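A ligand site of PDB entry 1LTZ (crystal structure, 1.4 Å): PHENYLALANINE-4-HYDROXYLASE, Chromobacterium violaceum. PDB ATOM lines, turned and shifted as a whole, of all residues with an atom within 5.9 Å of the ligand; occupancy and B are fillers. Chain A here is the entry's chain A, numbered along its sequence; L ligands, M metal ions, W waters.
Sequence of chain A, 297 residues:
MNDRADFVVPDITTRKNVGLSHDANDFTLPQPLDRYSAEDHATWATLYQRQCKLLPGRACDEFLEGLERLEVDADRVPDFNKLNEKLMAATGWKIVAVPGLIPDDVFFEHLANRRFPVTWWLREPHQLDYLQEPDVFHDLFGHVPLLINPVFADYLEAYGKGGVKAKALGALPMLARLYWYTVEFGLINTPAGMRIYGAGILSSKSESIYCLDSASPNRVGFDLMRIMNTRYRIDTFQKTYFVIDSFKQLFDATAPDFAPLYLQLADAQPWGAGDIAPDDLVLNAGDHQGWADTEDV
The backbone carbonyl oxygen of Gly 100 lies within hydrogen-bond range of a nitrogen (N2) of the ligand (3.1 Å). The backbone NH (N) of Ile 102 sits at hydrogen-bond distance from a nitrogen (N1) of the ligand. An oxygen (O3) of the ligand sits at hydrogen-bond distance from the side-chain carboxylate of Asp 104. O of Ile 102 is in hydrogen-bond range of N4 of the ligand (3.0 Å).
The backbone NH (N) of Val 98 lies within hydrogen-bond range of the backbone carbonyl oxygen (O) of Val 118 (3.0 Å). N of Glu 184 sits at hydrogen-bond distance from O of Tyr 179, 3.1 Å away. OH of Tyr 159 lies within hydrogen-bond range of O of Leu 175 (2.8 Å).
Merely in contact with the ligand: Phe 107, Tyr 159, Leu 101, Tyr 179, Val 98 and Glu 184. Hydrophobic or aromatic side chains within 4 Å of the ligand: Val 98, Leu 101, Ile 102, Phe 107 and Tyr 179. Within 4 Å of the ligand: Val 98, Gly 100, Leu 101, Ile 102, Asp 104, Phe 107, Tyr 159, Tyr 179 and Glu 184.
Water W4 bridges OH of Tyr 179 and O1 of the ligand. Water W1 lies within hydrogen-bond range of the side-chain carboxylate (OD2) of Asp 139 (2.4 Å), a nitrogen (N2) of the ligand (2.7 Å) and the side-chain hydroxyl (OG1) of Thr 119 (2.9 Å). Water W6 bridges the side-chain carboxylate of Asp 139 (2.7 Å) and an oxygen (O1) of the ligand (2.9 Å). Water W2 lies within hydrogen-bond range of O of Pro 117 (2.6 Å), N3 of the ligand (3.0 Å) and OD1 of Asp 139 (3.2 Å). Water W5 lies within hydrogen-bond range of the backbone carbonyl oxygen (O) of Leu 172 (2.8 Å), the side-chain carboxylate (OD2) of Asp 104 (2.9 Å) and an oxygen (O3) of the ligand (3.0 Å).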
ATOM      1  N   VAL A  98       5.739  -2.114  36.823  1.00  0.00           N
ATOM      2  CA  VAL A  98       7.005  -1.657  37.446  1.00  0.00           C
ATOM      3  C   VAL A  98       6.990  -0.133  37.442  1.00  0.00           C
ATOM      4  O   VAL A  98       6.251   0.526  36.675  1.00  0.00           O
ATOM      5  CB  VAL A  98       8.258  -2.270  36.815  1.00  0.00           C
ATOM      6  CG1 VAL A  98       8.224  -3.780  37.080  1.00  0.00           C
ATOM      7  CG2 VAL A  98       8.407  -1.998  35.328  1.00  0.00           C
ATOM      8  N   GLY A 100       9.252   1.898  36.502  1.00  0.00           N
ATOM      9  CA  GLY A 100      10.090   2.444  35.429  1.00  0.00           C
ATOM     10  C   GLY A 100      11.236   1.441  35.198  1.00  0.00           C
ATOM     11  O   GLY A 100      11.003   0.240  35.417  1.00  0.00           O
ATOM     12  N   LEU A 101      12.403   1.907  34.797  1.00  0.00           N
ATOM     13  CA  LEU A 101      13.557   1.028  34.595  1.00  0.00           C
ATOM     14  C   LEU A 101      13.908   0.265  35.875  1.00  0.00           C
ATOM     15  O   LEU A 101      13.927   0.883  36.933  1.00  0.00           O
ATOM     16  CB  LEU A 101      14.800   1.813  34.137  1.00  0.00           C
ATOM     17  CG  LEU A 101      14.769   2.205  32.655  1.00  0.00           C
ATOM     18  CD1 LEU A 101      15.877   3.223  32.355  1.00  0.00           C
ATOM     19  CD2 LEU A 101      14.887   0.978  31.763  1.00  0.00           C
ATOM     20  N   ILE A 102      14.168  -1.046  35.768  1.00  0.00           N
ATOM     21  CA  ILE A 102      14.529  -1.858  36.938  1.00  0.00           C
ATOM     22  C   ILE A 102      15.896  -2.478  36.710  1.00  0.00           C
ATOM     23  O   ILE A 102      16.394  -2.563  35.563  1.00  0.00           O
ATOM     24  CB  ILE A 102      13.478  -2.970  37.162  1.00  0.00           C
ATOM     25  CG1 ILE A 102      13.425  -4.018  36.059  1.00  0.00           C
ATOM     26  CG2 ILE A 102      12.123  -2.344  37.394  1.00  0.00           C
ATOM     27  CD1 ILE A 102      12.280  -5.023  36.122  1.00  0.00           C
ATOM     28  N   PRO A 103      16.551  -2.968  37.755  1.00  0.00           N
ATOM     29  CA  PRO A 103      17.887  -3.569  37.562  1.00  0.00           C
ATOM     30  C   PRO A 103      17.869  -4.707  36.566  1.00  0.00           C
ATOM     31  O   PRO A 103      16.912  -5.484  36.478  1.00  0.00           O
ATOM     32  CB  PRO A 103      18.226  -4.100  38.964  1.00  0.00           C
ATOM     33  CG  PRO A 103      17.489  -3.131  39.847  1.00  0.00           C
ATOM     34  CD  PRO A 103      16.148  -3.039  39.169  1.00  0.00           C
ATOM     35  N   ASP A 104      18.966  -4.823  35.815  1.00  0.00           N
ATOM     36  CA  ASP A 104      19.104  -5.866  34.800  1.00  0.00           C
ATOM     37  C   ASP A 104      18.819  -7.252  35.370  1.00  0.00           C
ATOM     38  O   ASP A 104      18.103  -8.009  34.715  1.00  0.00           O
ATOM     39  CB  ASP A 104      20.504  -5.896  34.183  1.00  0.00           C
ATOM     40  CG  ASP A 104      20.901  -4.720  33.308  1.00  0.00           C
ATOM     41  OD1 ASP A 104      20.118  -3.758  33.193  1.00  0.00           O
ATOM     42  OD2 ASP A 104      22.027  -4.770  32.732  1.00  0.00           O
ATOM     43  N   PHE A 107      15.072  -7.704  35.873  1.00  0.00           N
ATOM     44  CA  PHE A 107      14.522  -7.819  34.518  1.00  0.00           C
ATOM     45  C   PHE A 107      14.695  -9.212  33.936  1.00  0.00           C
ATOM     46  O   PHE A 107      13.703  -9.793  33.477  1.00  0.00           O
ATOM     47  CB  PHE A 107      15.212  -6.779  33.639  1.00  0.00           C
ATOM     48  CG  PHE A 107      14.611  -6.697  32.261  1.00  0.00           C
ATOM     49  CD1 PHE A 107      13.426  -6.003  32.062  1.00  0.00           C
ATOM     50  CD2 PHE A 107      15.217  -7.269  31.164  1.00  0.00           C
ATOM     51  CE1 PHE A 107      12.853  -5.858  30.824  1.00  0.00           C
ATOM     52  CE2 PHE A 107      14.635  -7.166  29.912  1.00  0.00           C
ATOM     53  CZ  PHE A 107      13.452  -6.472  29.728  1.00  0.00           C
ATOM     54  N   PHE A 108      15.900  -9.772  33.932  1.00  0.00           N
ATOM     55  CA  PHE A 108      16.090 -11.112  33.413  1.00  0.00           C
ATOM     56  C   PHE A 108      15.247 -12.160  34.154  1.00  0.00           C
ATOM     57  O   PHE A 108      14.733 -13.080  33.538  1.00  0.00           O
ATOM     58  CB  PHE A 108      17.534 -11.541  33.549  1.00  0.00           C
ATOM     59  CG  PHE A 108      18.577 -10.738  32.803  1.00  0.00           C
ATOM     60  CD1 PHE A 108      19.811 -10.505  33.399  1.00  0.00           C
ATOM     61  CD2 PHE A 108      18.364 -10.219  31.543  1.00  0.00           C
ATOM     62  CE1 PHE A 108      20.795  -9.790  32.726  1.00  0.00           C
ATOM     63  CE2 PHE A 108      19.338  -9.498  30.888  1.00  0.00           C
ATOM     64  CZ  PHE A 108      20.560  -9.282  31.471  1.00  0.00           C
ATOM     65  N   PHE A 116       6.519 -10.018  31.747  1.00  0.00           N
ATOM     66  CA  PHE A 116       7.034  -8.895  31.001  1.00  0.00           C
ATOM     67  C   PHE A 116       6.826  -7.626  31.810  1.00  0.00           C
ATOM     68  O   PHE A 116       5.656  -7.205  32.013  1.00  0.00           O
ATOM     69  CB  PHE A 116       6.445  -8.811  29.592  1.00  0.00           C
ATOM     70  CG  PHE A 116       7.237  -7.811  28.765  1.00  0.00           C
ATOM     71  CD1 PHE A 116       8.351  -8.282  28.105  1.00  0.00           C
ATOM     72  CD2 PHE A 116       6.894  -6.469  28.687  1.00  0.00           C
ATOM     73  CE1 PHE A 116       9.148  -7.413  27.383  1.00  0.00           C
ATOM     74  CE2 PHE A 116       7.689  -5.609  27.980  1.00  0.00           C
ATOM     75  CZ  PHE A 116       8.831  -6.073  27.321  1.00  0.00           C
ATOM     76  N   PRO A 117       7.886  -7.001  32.279  1.00  0.00           N
ATOM     77  CA  PRO A 117       7.715  -5.776  33.066  1.00  0.00           C
ATOM     78  C   PRO A 117       7.295  -4.580  32.187  1.00  0.00           C
ATOM     79  O   PRO A 117       7.938  -4.309  31.193  1.00  0.00           O
ATOM     80  CB  PRO A 117       9.097  -5.498  33.657  1.00  0.00           C
ATOM     81  CG  PRO A 117       9.863  -6.767  33.503  1.00  0.00           C
ATOM     82  CD  PRO A 117       9.297  -7.402  32.249  1.00  0.00           C
ATOM     83  N   VAL A 118       6.222  -3.907  32.643  1.00  0.00           N
ATOM     84  CA  VAL A 118       5.669  -2.738  31.967  1.00  0.00           C
ATOM     85  C   VAL A 118       5.674  -1.510  32.845  1.00  0.00           C
ATOM     86  O   VAL A 118       5.058  -1.526  33.924  1.00  0.00           O
ATOM     87  CB  VAL A 118       4.233  -3.056  31.506  1.00  0.00           C
ATOM     88  CG1 VAL A 118       3.566  -1.841  30.916  1.00  0.00           C
ATOM     89  CG2 VAL A 118       4.249  -4.203  30.497  1.00  0.00           C
ATOM     90  N   THR A 119       6.358  -0.455  32.412  1.00  0.00           N
ATOM     91  CA  THR A 119       6.274   0.801  33.177  1.00  0.00           C
ATOM     92  C   THR A 119       4.826   1.270  33.244  1.00  0.00           C
ATOM     93  O   THR A 119       4.216   1.392  32.177  1.00  0.00           O
ATOM     94  CB  THR A 119       7.118   1.860  32.443  1.00  0.00           C
ATOM     95  OG1 THR A 119       8.495   1.451  32.519  1.00  0.00           O
ATOM     96  CG2 THR A 119       6.976   3.220  33.120  1.00  0.00           C
ATOM     97  N   PRO A 134      11.380   3.804  28.902  1.00  0.00           N
ATOM     98  CA  PRO A 134      10.071   3.269  28.580  1.00  0.00           C
ATOM     99  C   PRO A 134       8.943   3.984  29.356  1.00  0.00           C
ATOM    100  O   PRO A 134       9.128   4.505  30.453  1.00  0.00           O
ATOM    101  CB  PRO A 134      10.203   1.833  29.075  1.00  0.00           C
ATOM    102  CG  PRO A 134      11.626   1.559  29.296  1.00  0.00           C
ATOM    103  CD  PRO A 134      12.347   2.870  29.473  1.00  0.00           C
ATOM    104  N   ASP A 139       5.819   0.227  26.271  1.00  0.00           N
ATOM    105  CA  ASP A 139       5.927  -1.176  26.713  1.00  0.00           C
ATOM    106  C   ASP A 139       4.732  -2.011  26.272  1.00  0.00           C
ATOM    107  O   ASP A 139       4.864  -3.126  25.738  1.00  0.00           O
ATOM    108  CB  ASP A 139       6.065  -1.200  28.247  1.00  0.00           C
ATOM    109  CG  ASP A 139       7.489  -1.023  28.707  1.00  0.00           C
ATOM    110  OD1 ASP A 139       8.412  -1.209  27.892  1.00  0.00           O
ATOM    111  OD2 ASP A 139       7.701  -0.668  29.912  1.00  0.00           O
ATOM    112  N   HIS A 143       5.982  -3.558  22.821  1.00  0.00           N
ATOM    113  CA  HIS A 143       6.592  -4.843  23.147  1.00  0.00           C
ATOM    114  C   HIS A 143       5.633  -6.005  23.224  1.00  0.00           C
ATOM    115  O   HIS A 143       5.882  -7.122  22.749  1.00  0.00           O
ATOM    116  CB  HIS A 143       7.289  -4.771  24.533  1.00  0.00           C
ATOM    117  CG  HIS A 143       8.650  -4.148  24.567  1.00  0.00           C
ATOM    118  ND1 HIS A 143       9.754  -4.850  24.105  1.00  0.00           N
ATOM    119  CD2 HIS A 143       9.138  -2.974  25.041  1.00  0.00           C
ATOM    120  CE1 HIS A 143      10.869  -4.083  24.279  1.00  0.00           C
ATOM    121  NE2 HIS A 143      10.519  -2.927  24.839  1.00  0.00           N
ATOM    122  N   TYR A 159      16.203 -15.719  26.357  1.00  0.00           N
ATOM    123  CA  TYR A 159      17.069 -14.561  26.619  1.00  0.00           C
ATOM    124  C   TYR A 159      17.150 -14.339  28.132  1.00  0.00           C
ATOM    125  O   TYR A 159      18.196 -14.140  28.739  1.00  0.00           O
ATOM    126  CB  TYR A 159      16.513 -13.315  25.873  1.00  0.00           C
ATOM    127  CG  TYR A 159      17.274 -12.069  26.235  1.00  0.00           C
ATOM    128  CD1 TYR A 159      18.450 -11.710  25.551  1.00  0.00           C
ATOM    129  CD2 TYR A 159      16.858 -11.230  27.253  1.00  0.00           C
ATOM    130  CE1 TYR A 159      19.113 -10.558  25.928  1.00  0.00           C
ATOM    131  CE2 TYR A 159      17.512 -10.104  27.660  1.00  0.00           C
ATOM    132  CZ  TYR A 159      18.650  -9.782  26.967  1.00  0.00           C
ATOM    133  OH  TYR A 159      19.293  -8.641  27.363  1.00  0.00           O
ATOM    134  N   LEU A 172      26.966  -8.262  30.826  1.00  0.00           N
ATOM    135  CA  LEU A 172      25.785  -7.370  30.847  1.00  0.00           C
ATOM    136  C   LEU A 172      25.715  -6.420  29.685  1.00  0.00           C
ATOM    137  O   LEU A 172      24.669  -6.350  29.018  1.00  0.00           O
ATOM    138  CB  LEU A 172      25.744  -6.693  32.239  1.00  0.00           C
ATOM    139  CG  LEU A 172      25.479  -7.656  33.403  1.00  0.00           C
ATOM    140  CD1 LEU A 172      25.504  -6.874  34.707  1.00  0.00           C
ATOM    141  CD2 LEU A 172      24.170  -8.417  33.270  1.00  0.00           C
ATOM    142  N   LEU A 175      24.700  -8.518  26.542  1.00  0.00           N
ATOM    143  CA  LEU A 175      23.270  -8.862  26.540  1.00  0.00           C
ATOM    144  C   LEU A 175      22.397  -7.643  26.317  1.00  0.00           C
ATOM    145  O   LEU A 175      21.321  -7.723  25.718  1.00  0.00           O
ATOM    146  CB  LEU A 175      22.905  -9.518  27.879  1.00  0.00           C
ATOM    147  CG  LEU A 175      23.470 -10.926  28.066  1.00  0.00           C
ATOM    148  CD1 LEU A 175      23.170 -11.441  29.461  1.00  0.00           C
ATOM    149  CD2 LEU A 175      22.893 -11.891  27.023  1.00  0.00           C
ATOM    150  N   ALA A 176      22.783  -6.481  26.809  1.00  0.00           N
ATOM    151  CA  ALA A 176      22.047  -5.240  26.512  1.00  0.00           C
ATOM    152  C   ALA A 176      22.047  -4.898  25.032  1.00  0.00           C
ATOM    153  O   ALA A 176      21.026  -4.492  24.468  1.00  0.00           O
ATOM    154  CB  ALA A 176      22.632  -4.104  27.306  1.00  0.00           C
ATOM    155  N   TYR A 179      19.722  -7.349  23.194  1.00  0.00           N
ATOM    156  CA  TYR A 179      18.294  -6.963  23.357  1.00  0.00           C
ATOM    157  C   TYR A 179      17.968  -5.722  22.541  1.00  0.00           C
ATOM    158  O   TYR A 179      16.929  -5.634  21.859  1.00  0.00           O
ATOM    159  CB  TYR A 179      18.045  -6.725  24.850  1.00  0.00           C
ATOM    160  CG  TYR A 179      16.593  -6.602  25.263  1.00  0.00           C
ATOM    161  CD1 TYR A 179      15.863  -7.735  25.551  1.00  0.00           C
ATOM    162  CD2 TYR A 179      15.893  -5.382  25.390  1.00  0.00           C
ATOM    163  CE1 TYR A 179      14.542  -7.732  25.931  1.00  0.00           C
ATOM    164  CE2 TYR A 179      14.539  -5.383  25.775  1.00  0.00           C
ATOM    165  CZ  TYR A 179      13.867  -6.549  26.038  1.00  0.00           C
ATOM    166  OH  TYR A 179      12.542  -6.576  26.440  1.00  0.00           O
ATOM    167  N   GLU A 184      14.360  -4.331  20.748  1.00  0.00           N
ATOM    168  CA  GLU A 184      14.049  -2.903  20.680  1.00  0.00           C
ATOM    169  C   GLU A 184      14.078  -2.358  19.234  1.00  0.00           C
ATOM    170  O   GLU A 184      13.161  -1.580  18.903  1.00  0.00           O
ATOM    171  CB  GLU A 184      14.953  -2.069  21.577  1.00  0.00           C
ATOM    172  CG  GLU A 184      14.891  -2.422  23.061  1.00  0.00           C
ATOM    173  CD  GLU A 184      13.659  -1.971  23.807  1.00  0.00           C
ATOM    174  OE1 GLU A 184      12.718  -1.344  23.276  1.00  0.00           O
ATOM    175  OE2 GLU A 184      13.563  -2.268  25.040  1.00  0.00           O
ATOM    176  N   TYR A 232      25.672   0.951  20.825  1.00  0.00           N
ATOM    177  CA  TYR A 232      24.457   1.610  20.401  1.00  0.00           C
ATOM    178  C   TYR A 232      24.362   2.969  21.105  1.00  0.00           C
ATOM    179  O   TYR A 232      25.021   3.228  22.135  1.00  0.00           O
ATOM    180  CB  TYR A 232      23.209   0.767  20.658  1.00  0.00           C
ATOM    181  CG  TYR A 232      22.855   0.499  22.081  1.00  0.00           C
ATOM    182  CD1 TYR A 232      22.128   1.344  22.910  1.00  0.00           C
ATOM    183  CD2 TYR A 232      23.262  -0.727  22.632  1.00  0.00           C
ATOM    184  CE1 TYR A 232      21.795   1.090  24.229  1.00  0.00           C
ATOM    185  CE2 TYR A 232      22.946  -1.024  23.954  1.00  0.00           C
ATOM    186  CZ  TYR A 232      22.223  -0.127  24.740  1.00  0.00           C
ATOM    187  OH  TYR A 232      21.952  -0.496  26.031  1.00  0.00           O
HETATM  188  N1  LIG L   1      13.737  -2.401  32.923  1.00  0.00           N
HETATM  189  N2  LIG L   1      11.458  -1.803  33.120  1.00  0.00           N
HETATM  190  C1  LIG L   1      12.522  -2.186  32.369  1.00  0.00           C
HETATM  191  N3  LIG L   1      12.338  -2.305  31.013  1.00  0.00           N
HETATM  192  C2  LIG L   1      13.354  -2.590  30.158  1.00  0.00           C
HETATM  193  O1  LIG L   1      13.191  -2.622  28.914  1.00  0.00           O
HETATM  194  C3  LIG L   1      14.676  -2.809  30.679  1.00  0.00           C
HETATM  195  C4  LIG L   1      14.787  -2.713  32.112  1.00  0.00           C
HETATM  196  N4  LIG L   1      16.018  -2.960  32.663  1.00  0.00           N
HETATM  197  C5  LIG L   1      16.992  -3.636  31.915  1.00  0.00           C
HETATM  198  C6  LIG L   1      17.036  -3.340  30.455  1.00  0.00           C
HETATM  199  N5  LIG L   1      15.778  -2.979  29.853  1.00  0.00           N
HETATM  200  C7  LIG L   1      18.271  -3.282  29.531  1.00  0.00           C
HETATM  201  O2  LIG L   1      19.315  -2.506  30.214  1.00  0.00           O
HETATM  202  C8  LIG L   1      18.887  -4.643  29.201  1.00  0.00           C
HETATM  203  O3  LIG L   1      19.415  -5.221  30.439  1.00  0.00           O
HETATM  204  C9  LIG L   1      17.840  -5.568  28.637  1.00  0.00           C
HETATM  205 FE    FE M   1      11.706  -1.189  25.270  1.00  0.00          FE
HETATM  206  O   HOH W   1       9.512  -1.083  31.470  1.00  0.00           O
HETATM  207  O   HOH W   2       9.885  -3.405  29.692  1.00  0.00           O
HETATM  208  O   HOH W   3      15.741  -2.144  26.995  1.00  0.00           O
HETATM  209  O   HOH W   4      11.768  -4.402  27.619  1.00  0.00           O
HETATM  210  O   HOH W   5      22.220  -6.345  30.361  1.00  0.00           O
HETATM  211  O   HOH W   6      11.096  -1.298  27.389  1.00  0.00           O
HETATM  212  O   HOH W   7      22.278  -1.108  29.676  1.00  0.00           O
HETATM  213  O   HOH W   8      14.613   0.345  27.848  1.00  0.00           O
